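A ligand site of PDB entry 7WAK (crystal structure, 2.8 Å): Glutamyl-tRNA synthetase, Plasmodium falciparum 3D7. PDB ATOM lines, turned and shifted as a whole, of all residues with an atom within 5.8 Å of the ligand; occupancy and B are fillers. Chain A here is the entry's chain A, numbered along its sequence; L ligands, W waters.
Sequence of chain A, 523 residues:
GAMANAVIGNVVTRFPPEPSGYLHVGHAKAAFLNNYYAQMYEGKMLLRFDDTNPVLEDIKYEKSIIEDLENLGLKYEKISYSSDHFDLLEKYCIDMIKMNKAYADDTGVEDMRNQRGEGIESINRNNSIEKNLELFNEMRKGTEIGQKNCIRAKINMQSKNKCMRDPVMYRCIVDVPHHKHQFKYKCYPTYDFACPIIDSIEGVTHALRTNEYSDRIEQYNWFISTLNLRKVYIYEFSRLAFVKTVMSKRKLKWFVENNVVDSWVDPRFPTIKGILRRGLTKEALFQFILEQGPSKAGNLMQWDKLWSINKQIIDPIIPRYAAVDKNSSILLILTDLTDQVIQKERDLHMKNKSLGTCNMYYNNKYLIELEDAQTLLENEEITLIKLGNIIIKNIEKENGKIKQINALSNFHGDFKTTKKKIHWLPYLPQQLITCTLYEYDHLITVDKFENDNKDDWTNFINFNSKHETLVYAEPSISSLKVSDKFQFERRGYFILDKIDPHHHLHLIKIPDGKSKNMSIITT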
ATOM      1  N   ARG A  14      10.446 -28.881  -8.608  1.00  0.00           N
ATOM      2  CA  ARG A  14      10.970 -27.922  -7.641  1.00  0.00           C
ATOM      3  C   ARG A  14      12.344 -27.422  -8.058  1.00  0.00           C
ATOM      4  O   ARG A  14      13.106 -28.094  -8.751  1.00  0.00           O
ATOM      5  CB  ARG A  14      11.095 -28.506  -6.214  1.00  0.00           C
ATOM      6  CG  ARG A  14      12.407 -29.281  -5.985  1.00  0.00           C
ATOM      7  CD  ARG A  14      12.380 -30.542  -6.824  1.00  0.00           C
ATOM      8  NE  ARG A  14      13.512 -31.420  -6.660  1.00  0.00           N
ATOM      9  CZ  ARG A  14      14.594 -31.371  -7.417  1.00  0.00           C
ATOM     10  NH1 ARG A  14      14.676 -30.464  -8.389  1.00  0.00           N
ATOM     11  NH2 ARG A  14      15.586 -32.239  -7.228  1.00  0.00           N
ATOM     12  N   PHE A  15      12.649 -26.217  -7.566  1.00  0.00           N
ATOM     13  CA  PHE A  15      13.919 -25.552  -7.745  1.00  0.00           C
ATOM     14  C   PHE A  15      14.644 -25.553  -6.405  1.00  0.00           C
ATOM     15  O   PHE A  15      14.114 -25.003  -5.429  1.00  0.00           O
ATOM     16  CB  PHE A  15      13.690 -24.116  -8.249  1.00  0.00           C
ATOM     17  CG  PHE A  15      14.949 -23.362  -8.472  1.00  0.00           C
ATOM     18  CD1 PHE A  15      16.015 -23.961  -9.155  1.00  0.00           C
ATOM     19  CD2 PHE A  15      15.100 -22.058  -7.976  1.00  0.00           C
ATOM     20  CE1 PHE A  15      17.214 -23.276  -9.353  1.00  0.00           C
ATOM     21  CE2 PHE A  15      16.300 -21.353  -8.174  1.00  0.00           C
ATOM     22  CZ  PHE A  15      17.366 -21.972  -8.857  1.00  0.00           C
ATOM     23  N   PRO A  16      15.794 -26.192  -6.281  1.00  0.00           N
ATOM     24  CA  PRO A  16      16.333 -26.475  -4.948  1.00  0.00           C
ATOM     25  C   PRO A  16      17.705 -25.859  -4.736  1.00  0.00           C
ATOM     26  O   PRO A  16      18.665 -26.596  -4.476  1.00  0.00           O
ATOM     27  CB  PRO A  16      16.431 -28.004  -4.941  1.00  0.00           C
ATOM     28  CG  PRO A  16      16.905 -28.307  -6.379  1.00  0.00           C
ATOM     29  CD  PRO A  16      16.363 -27.132  -7.273  1.00  0.00           C
ATOM     30  N   PRO A  17      17.841 -24.540  -4.824  1.00  0.00           N
ATOM     31  CA  PRO A  17      19.164 -23.927  -4.708  1.00  0.00           C
ATOM     32  C   PRO A  17      19.623 -23.828  -3.267  1.00  0.00           C
ATOM     33  O   PRO A  17      18.810 -23.801  -2.338  1.00  0.00           O
ATOM     34  CB  PRO A  17      18.935 -22.522  -5.292  1.00  0.00           C
ATOM     35  CG  PRO A  17      17.531 -22.202  -4.852  1.00  0.00           C
ATOM     36  CD  PRO A  17      16.775 -23.520  -4.908  1.00  0.00           C
ATOM     37  N   GLU A  18      20.912 -23.754  -3.091  1.00  0.00           N
ATOM     38  CA  GLU A  18      21.414 -23.576  -1.731  1.00  0.00           C
ATOM     39  C   GLU A  18      21.555 -22.106  -1.405  1.00  0.00           C
ATOM     40  O   GLU A  18      22.131 -21.352  -2.210  1.00  0.00           O
ATOM     41  CB  GLU A  18      22.767 -24.241  -1.538  1.00  0.00           C
ATOM     42  CG  GLU A  18      22.845 -25.709  -1.843  1.00  0.00           C
ATOM     43  CD  GLU A  18      24.282 -26.206  -1.744  1.00  0.00           C
ATOM     44  OE1 GLU A  18      25.099 -25.474  -1.124  1.00  0.00           O
ATOM     45  OE2 GLU A  18      24.575 -27.288  -2.302  1.00  0.00           O
ATOM     46  N   HIS A  24      23.475 -17.367 -10.552  1.00  0.00           N
ATOM     47  CA  HIS A  24      24.132 -17.043 -11.807  1.00  0.00           C
ATOM     48  C   HIS A  24      23.268 -17.588 -12.962  1.00  0.00           C
ATOM     49  O   HIS A  24      22.138 -18.042 -12.754  1.00  0.00           O
ATOM     50  CB  HIS A  24      25.560 -17.572 -11.793  1.00  0.00           C
ATOM     51  CG  HIS A  24      25.667 -19.058 -11.621  1.00  0.00           C
ATOM     52  ND1 HIS A  24      25.567 -19.945 -12.671  1.00  0.00           N
ATOM     53  CD2 HIS A  24      25.881 -19.809 -10.508  1.00  0.00           C
ATOM     54  CE1 HIS A  24      25.716 -21.173 -12.217  1.00  0.00           C
ATOM     55  NE2 HIS A  24      25.895 -21.119 -10.910  1.00  0.00           N
ATOM     56  N   VAL A  25      23.810 -17.565 -14.185  1.00  0.00           N
ATOM     57  CA  VAL A  25      22.980 -17.880 -15.348  1.00  0.00           C
ATOM     58  C   VAL A  25      22.572 -19.353 -15.342  1.00  0.00           C
ATOM     59  O   VAL A  25      21.421 -19.689 -15.630  1.00  0.00           O
ATOM     60  CB  VAL A  25      23.694 -17.497 -16.665  1.00  0.00           C
ATOM     61  CG1 VAL A  25      23.513 -16.045 -16.970  1.00  0.00           C
ATOM     62  CG2 VAL A  25      25.173 -17.875 -16.625  1.00  0.00           C
ATOM     63  N   GLY A  26      23.525 -20.270 -15.083  1.00  0.00           N
ATOM     64  CA  GLY A  26      23.189 -21.693 -15.083  1.00  0.00           C
ATOM     65  C   GLY A  26      22.045 -22.018 -14.126  1.00  0.00           C
ATOM     66  O   GLY A  26      21.119 -22.793 -14.450  1.00  0.00           O
ATOM     67  N   HIS A  27      22.083 -21.428 -12.934  1.00  0.00           N
ATOM     68  CA  HIS A  27      20.920 -21.465 -12.074  1.00  0.00           C
ATOM     69  C   HIS A  27      19.660 -21.053 -12.829  1.00  0.00           C
ATOM     70  O   HIS A  27      18.605 -21.677 -12.666  1.00  0.00           O
ATOM     71  CB  HIS A  27      21.127 -20.573 -10.849  1.00  0.00           C
ATOM     72  CG  HIS A  27      22.167 -21.082  -9.905  1.00  0.00           C
ATOM     73  ND1 HIS A  27      23.030 -20.249  -9.228  1.00  0.00           N
ATOM     74  CD2 HIS A  27      22.476 -22.340  -9.509  1.00  0.00           C
ATOM     75  CE1 HIS A  27      23.816 -20.964  -8.458  1.00  0.00           C
ATOM     76  NE2 HIS A  27      23.509 -22.240  -8.617  1.00  0.00           N
ATOM     77  N   LYS A  29      18.925 -21.348 -16.009  1.00  0.00           N
ATOM     78  CA  LYS A  29      18.434 -22.462 -16.826  1.00  0.00           C
ATOM     79  C   LYS A  29      17.639 -23.458 -15.992  1.00  0.00           C
ATOM     80  O   LYS A  29      16.524 -23.835 -16.362  1.00  0.00           O
ATOM     81  CB  LYS A  29      19.570 -23.192 -17.548  1.00  0.00           C
ATOM     82  CG  LYS A  29      19.066 -24.328 -18.442  1.00  0.00           C
ATOM     83  CD  LYS A  29      20.177 -25.319 -18.804  1.00  0.00           C
ATOM     84  CE  LYS A  29      20.044 -25.816 -20.237  1.00  0.00           C
ATOM     85  NZ  LYS A  29      20.701 -27.136 -20.435  1.00  0.00           N
ATOM     86  N   ALA A  30      18.217 -23.906 -14.863  1.00  0.00           N
ATOM     87  CA  ALA A  30      17.507 -24.881 -14.038  1.00  0.00           C
ATOM     88  C   ALA A  30      16.150 -24.340 -13.587  1.00  0.00           C
ATOM     89  O   ALA A  30      15.121 -25.030 -13.672  1.00  0.00           O
ATOM     90  CB  ALA A  30      18.326 -25.254 -12.808  1.00  0.00           C
ATOM     91  N   ASN A  34      12.507 -26.046 -14.740  1.00  0.00           N
ATOM     92  CA  ASN A  34      11.498 -26.440 -13.774  1.00  0.00           C
ATOM     93  C   ASN A  34      10.179 -25.736 -14.029  1.00  0.00           C
ATOM     94  O   ASN A  34       9.106 -26.364 -14.037  1.00  0.00           O
ATOM     95  CB  ASN A  34      11.956 -26.161 -12.360  1.00  0.00           C
ATOM     96  CG  ASN A  34      12.902 -27.202 -11.838  1.00  0.00           C
ATOM     97  OD1 ASN A  34      12.554 -28.382 -11.746  1.00  0.00           O
ATOM     98  ND2 ASN A  34      14.122 -26.764 -11.513  1.00  0.00           N
ATOM     99  N   ASP A  50      17.782 -25.321  -0.015  1.00  0.00           N
ATOM    100  CA  ASP A  50      18.437 -26.548   0.358  1.00  0.00           C
ATOM    101  C   ASP A  50      19.543 -26.234   1.356  1.00  0.00           C
ATOM    102  O   ASP A  50      20.713 -26.064   1.027  1.00  0.00           O
ATOM    103  CB  ASP A  50      18.922 -27.265  -0.881  1.00  0.00           C
ATOM    104  CG  ASP A  50      19.817 -28.391  -0.570  1.00  0.00           C
ATOM    105  OD1 ASP A  50      19.586 -29.047   0.473  1.00  0.00           O
ATOM    106  OD2 ASP A  50      20.750 -28.593  -1.360  1.00  0.00           O
ATOM    107  N   LEU A 208      14.305 -32.412 -11.419  1.00  0.00           N
ATOM    108  CA  LEU A 208      15.229 -32.032 -12.479  1.00  0.00           C
ATOM    109  C   LEU A 208      16.623 -31.897 -11.900  1.00  0.00           C
ATOM    110  O   LEU A 208      16.780 -31.200 -10.883  1.00  0.00           O
ATOM    111  CB  LEU A 208      14.812 -30.711 -13.133  1.00  0.00           C
ATOM    112  CG  LEU A 208      14.052 -30.839 -14.445  1.00  0.00           C
ATOM    113  CD1 LEU A 208      12.875 -31.752 -14.219  1.00  0.00           C
ATOM    114  CD2 LEU A 208      13.589 -29.514 -14.918  1.00  0.00           C
ATOM    115  N   ARG A 209      17.622 -32.554 -12.505  1.00  0.00           N
ATOM    116  CA  ARG A 209      18.998 -32.472 -12.016  1.00  0.00           C
ATOM    117  C   ARG A 209      19.988 -32.423 -13.180  1.00  0.00           C
ATOM    118  O   ARG A 209      19.760 -33.051 -14.216  1.00  0.00           O
ATOM    119  CB  ARG A 209      19.414 -33.637 -11.101  1.00  0.00           C
ATOM    120  CG  ARG A 209      18.309 -34.377 -10.378  1.00  0.00           C
ATOM    121  CD  ARG A 209      18.951 -35.462  -9.522  1.00  0.00           C
ATOM    122  NE  ARG A 209      19.821 -34.890  -8.501  1.00  0.00           N
ATOM    123  CZ  ARG A 209      20.474 -35.582  -7.577  1.00  0.00           C
ATOM    124  NH1 ARG A 209      20.372 -36.913  -7.550  1.00  0.00           N
ATOM    125  NH2 ARG A 209      21.234 -34.944  -6.690  1.00  0.00           N
ATOM    126  N   THR A 210      21.090 -31.700 -12.962  1.00  0.00           N
ATOM    127  CA  THR A 210      22.187 -31.645 -13.929  1.00  0.00           C
ATOM    128  C   THR A 210      22.736 -33.028 -14.176  1.00  0.00           C
ATOM    129  O   THR A 210      23.012 -33.783 -13.234  1.00  0.00           O
ATOM    130  CB  THR A 210      23.313 -30.744 -13.414  1.00  0.00           C
ATOM    131  OG1 THR A 210      23.493 -30.937 -11.998  1.00  0.00           O
ATOM    132  CG2 THR A 210      23.025 -29.283 -13.733  1.00  0.00           C
ATOM    133  N   PHE A 237      19.276 -32.824 -17.413  1.00  0.00           N
ATOM    134  CA  PHE A 237      19.549 -31.857 -18.462  1.00  0.00           C
ATOM    135  C   PHE A 237      21.019 -31.444 -18.374  1.00  0.00           C
ATOM    136  O   PHE A 237      21.685 -31.654 -17.349  1.00  0.00           O
ATOM    137  CB  PHE A 237      18.615 -30.632 -18.360  1.00  0.00           C
ATOM    138  CG  PHE A 237      18.713 -29.908 -17.056  1.00  0.00           C
ATOM    139  CD1 PHE A 237      17.756 -30.081 -16.088  1.00  0.00           C
ATOM    140  CD2 PHE A 237      19.762 -29.043 -16.790  1.00  0.00           C
ATOM    141  CE1 PHE A 237      17.850 -29.421 -14.877  1.00  0.00           C
ATOM    142  CE2 PHE A 237      19.873 -28.382 -15.569  1.00  0.00           C
ATOM    143  CZ  PHE A 237      18.921 -28.576 -14.610  1.00  0.00           C
ATOM    144  N   SER A 238      21.508 -30.847 -19.466  1.00  0.00           N
ATOM    145  CA  SER A 238      22.890 -30.368 -19.510  1.00  0.00           C
ATOM    146  C   SER A 238      23.038 -29.086 -18.682  1.00  0.00           C
ATOM    147  O   SER A 238      22.167 -28.212 -18.699  1.00  0.00           O
ATOM    148  CB  SER A 238      23.328 -30.090 -20.945  1.00  0.00           C
ATOM    149  OG  SER A 238      22.255 -29.536 -21.690  1.00  0.00           O
ATOM    150  N   ARG A 239      24.161 -29.010 -17.968  1.00  0.00           N
ATOM    151  CA  ARG A 239      24.580 -27.808 -17.250  1.00  0.00           C
ATOM    152  C   ARG A 239      25.001 -26.739 -18.240  1.00  0.00           C
ATOM    153  O   ARG A 239      25.542 -27.042 -19.307  1.00  0.00           O
ATOM    154  CB  ARG A 239      25.767 -28.167 -16.330  1.00  0.00           C
ATOM    155  CG  ARG A 239      25.901 -27.394 -15.052  1.00  0.00           C
ATOM    156  CD  ARG A 239      26.581 -28.201 -13.927  1.00  0.00           C
ATOM    157  NE  ARG A 239      25.931 -27.993 -12.621  1.00  0.00           N
ATOM    158  CZ  ARG A 239      25.980 -28.838 -11.599  1.00  0.00           C
ATOM    159  NH1 ARG A 239      26.668 -29.976 -11.716  1.00  0.00           N
ATOM    160  NH2 ARG A 239      25.351 -28.554 -10.456  1.00  0.00           N
ATOM    161  N   LEU A 240      24.770 -25.472 -17.880  1.00  0.00           N
ATOM    162  CA  LEU A 240      25.038 -24.331 -18.763  1.00  0.00           C
ATOM    163  C   LEU A 240      26.342 -23.632 -18.373  1.00  0.00           C
ATOM    164  O   LEU A 240      26.434 -23.034 -17.299  1.00  0.00           O
ATOM    165  CB  LEU A 240      23.871 -23.338 -18.708  1.00  0.00           C
ATOM    166  CG  LEU A 240      23.944 -22.016 -19.476  1.00  0.00           C
ATOM    167  CD1 LEU A 240      24.289 -22.220 -20.954  1.00  0.00           C
ATOM    168  CD2 LEU A 240      22.670 -21.182 -19.328  1.00  0.00           C
ATOM    169  N   ALA A 241      27.350 -23.676 -19.261  1.00  0.00           N
ATOM    170  CA  ALA A 241      28.632 -22.990 -19.033  1.00  0.00           C
ATOM    171  C   ALA A 241      29.025 -22.137 -20.230  1.00  0.00           C
ATOM    172  O   ALA A 241      28.828 -22.527 -21.390  1.00  0.00           O
ATOM    173  CB  ALA A 241      29.744 -23.975 -18.728  1.00  0.00           C
ATOM    174  N   MET A 247      32.236 -19.033 -13.019  1.00  0.00           N
ATOM    175  CA  MET A 247      31.110 -19.009 -12.105  1.00  0.00           C
ATOM    176  C   MET A 247      31.380 -19.724 -10.789  1.00  0.00           C
ATOM    177  O   MET A 247      30.457 -19.831  -9.964  1.00  0.00           O
ATOM    178  CB  MET A 247      29.863 -19.635 -12.763  1.00  0.00           C
ATOM    179  CG  MET A 247      29.579 -19.183 -14.209  1.00  0.00           C
ATOM    180  SD  MET A 247      28.291 -20.203 -15.020  1.00  0.00           S
ATOM    181  CE  MET A 247      28.940 -20.189 -16.698  1.00  0.00           C
HETATM  182  P1  LIG L   1      25.540 -25.998  -7.046  1.00  0.00           P
HETATM  183  O1  LIG L   1      25.764 -26.983  -8.117  1.00  0.00           O
HETATM  184  O2  LIG L   1      26.238 -26.402  -5.827  1.00  0.00           O
HETATM  185  O3  LIG L   1      25.727 -24.584  -7.371  1.00  0.00           O
HETATM  186  P2  LIG L   1      22.901 -25.310  -6.347  1.00  0.00           P
HETATM  187  O4  LIG L   1      22.391 -26.221  -5.410  1.00  0.00           O
HETATM  188  O5  LIG L   1      23.228 -23.997  -5.959  1.00  0.00           O
HETATM  189  O6  LIG L   1      24.043 -26.261  -6.727  1.00  0.00           O
HETATM  190  O7  LIG L   1      22.067 -25.378  -7.633  1.00  0.00           O
HETATM  191  C1  LIG L   1      20.679 -25.329  -7.660  1.00  0.00           C
HETATM  192  C2  LIG L   1      20.172 -25.855  -8.959  1.00  0.00           C
HETATM  193  O8  LIG L   1      20.884 -25.316 -10.015  1.00  0.00           O
HETATM  194  C3  LIG L   1      20.431 -27.296  -9.036  1.00  0.00           C
HETATM  195  O9  LIG L   1      19.278 -27.858  -9.597  1.00  0.00           O
HETATM  196  C4  LIG L   1      21.528 -27.371  -9.999  1.00  0.00           C
HETATM  197  O10 LIG L   1      21.568 -28.645 -10.549  1.00  0.00           O
HETATM  198  C5  LIG L   1      21.195 -26.277 -10.935  1.00  0.00           C
HETATM  199  N1  LIG L   1      22.389 -25.762 -11.522  1.00  0.00           N
HETATM  200  C6  LIG L   1      23.440 -25.448 -10.853  1.00  0.00           C
HETATM  201  N2  LIG L   1      24.407 -25.019 -11.625  1.00  0.00           N
HETATM  202  C7  LIG L   1      23.967 -25.042 -12.816  1.00  0.00           C
HETATM  203  C8  LIG L   1      24.473 -24.690 -14.111  1.00  0.00           C
HETATM  204  N3  LIG L   1      25.688 -24.226 -14.307  1.00  0.00           N
HETATM  205  N4  LIG L   1      23.712 -24.851 -15.136  1.00  0.00           N
HETATM  206  C9  LIG L   1      22.495 -25.287 -15.000  1.00  0.00           C
HETATM  207  N5  LIG L   1      21.983 -25.633 -13.857  1.00  0.00           N
HETATM  208  C10 LIG L   1      22.646 -25.530 -12.738  1.00  0.00           C
HETATM  209  O   HOH W   1      22.114 -31.674  -9.408  1.00  0.00           O
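NH1 of Arg 239 lies close to OG1 of Thr 210. The backbone NH of Gly 26 lies within hydrogen-bond range of a ring nitrogen (ND1) of His 24, 3.2 Å away. A ring nitrogen (ND1) of His 27 sits close to the backbone NH (N) of His 24 (3.2 Å). The backbone carbonyl oxygen of Ala 30 lies within hydrogen-bond range of the side-chain amide nitrogen of Asn 34 (2.9 Å). The backbone carbonyl oxygen of Pro 17 is in hydrogen-bond range of the backbone NH of Asp 50. A ring nitrogen (ND1) of His 24 is in hydrogen-bond range of the side-chain sulfur (SD) of Met 247 (3.6 Å). The backbone NH (N) of Phe 237 sits at hydrogen-bond distance from the backbone carbonyl oxygen (O) of Arg 209.
Water W1 bridges OG1 of Thr 210 and O10 of the ligand.
N5 of the ligand lies close to O of Gly 26. Phe 15 touches the ligand (CE1 to C2, 3.9 Å). Pro 16 touches the ligand (CD to O9, 3.8 Å). Pro 17 touches the ligand. Glu 18 touches the ligand. His 24 touches the ligand. Ala 30 touches the ligand (CB to C5, 3.6 Å). CE2 of Phe 237 touches N5 of the ligand, at 3.9 Å. Hydrophobic or aromatic side chains within 4 Å of the ligand: Phe 15, Pro 16, His 24, His 27, Ala 30, Phe 237 and Leu 240. The nearest printed residue that does not touch the ligand is Leu 208 (4.4 Å).
NH2 of Arg 239 lies within salt-bridge range of O1 of the ligand. N of Leu 240 sits at hydrogen-bond distance from N4 of the ligand (3.0 Å). O of Leu 240 sits at hydrogen-bond distance from N3 of the ligand (3.3 Å). An oxygen (O5) of the ligand is in hydrogen-bond range of a ring nitrogen (NE2) of His 27. OG1 of Thr 210 sits at hydrogen-bond distance from O10 of the ligand (3.3 Å).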
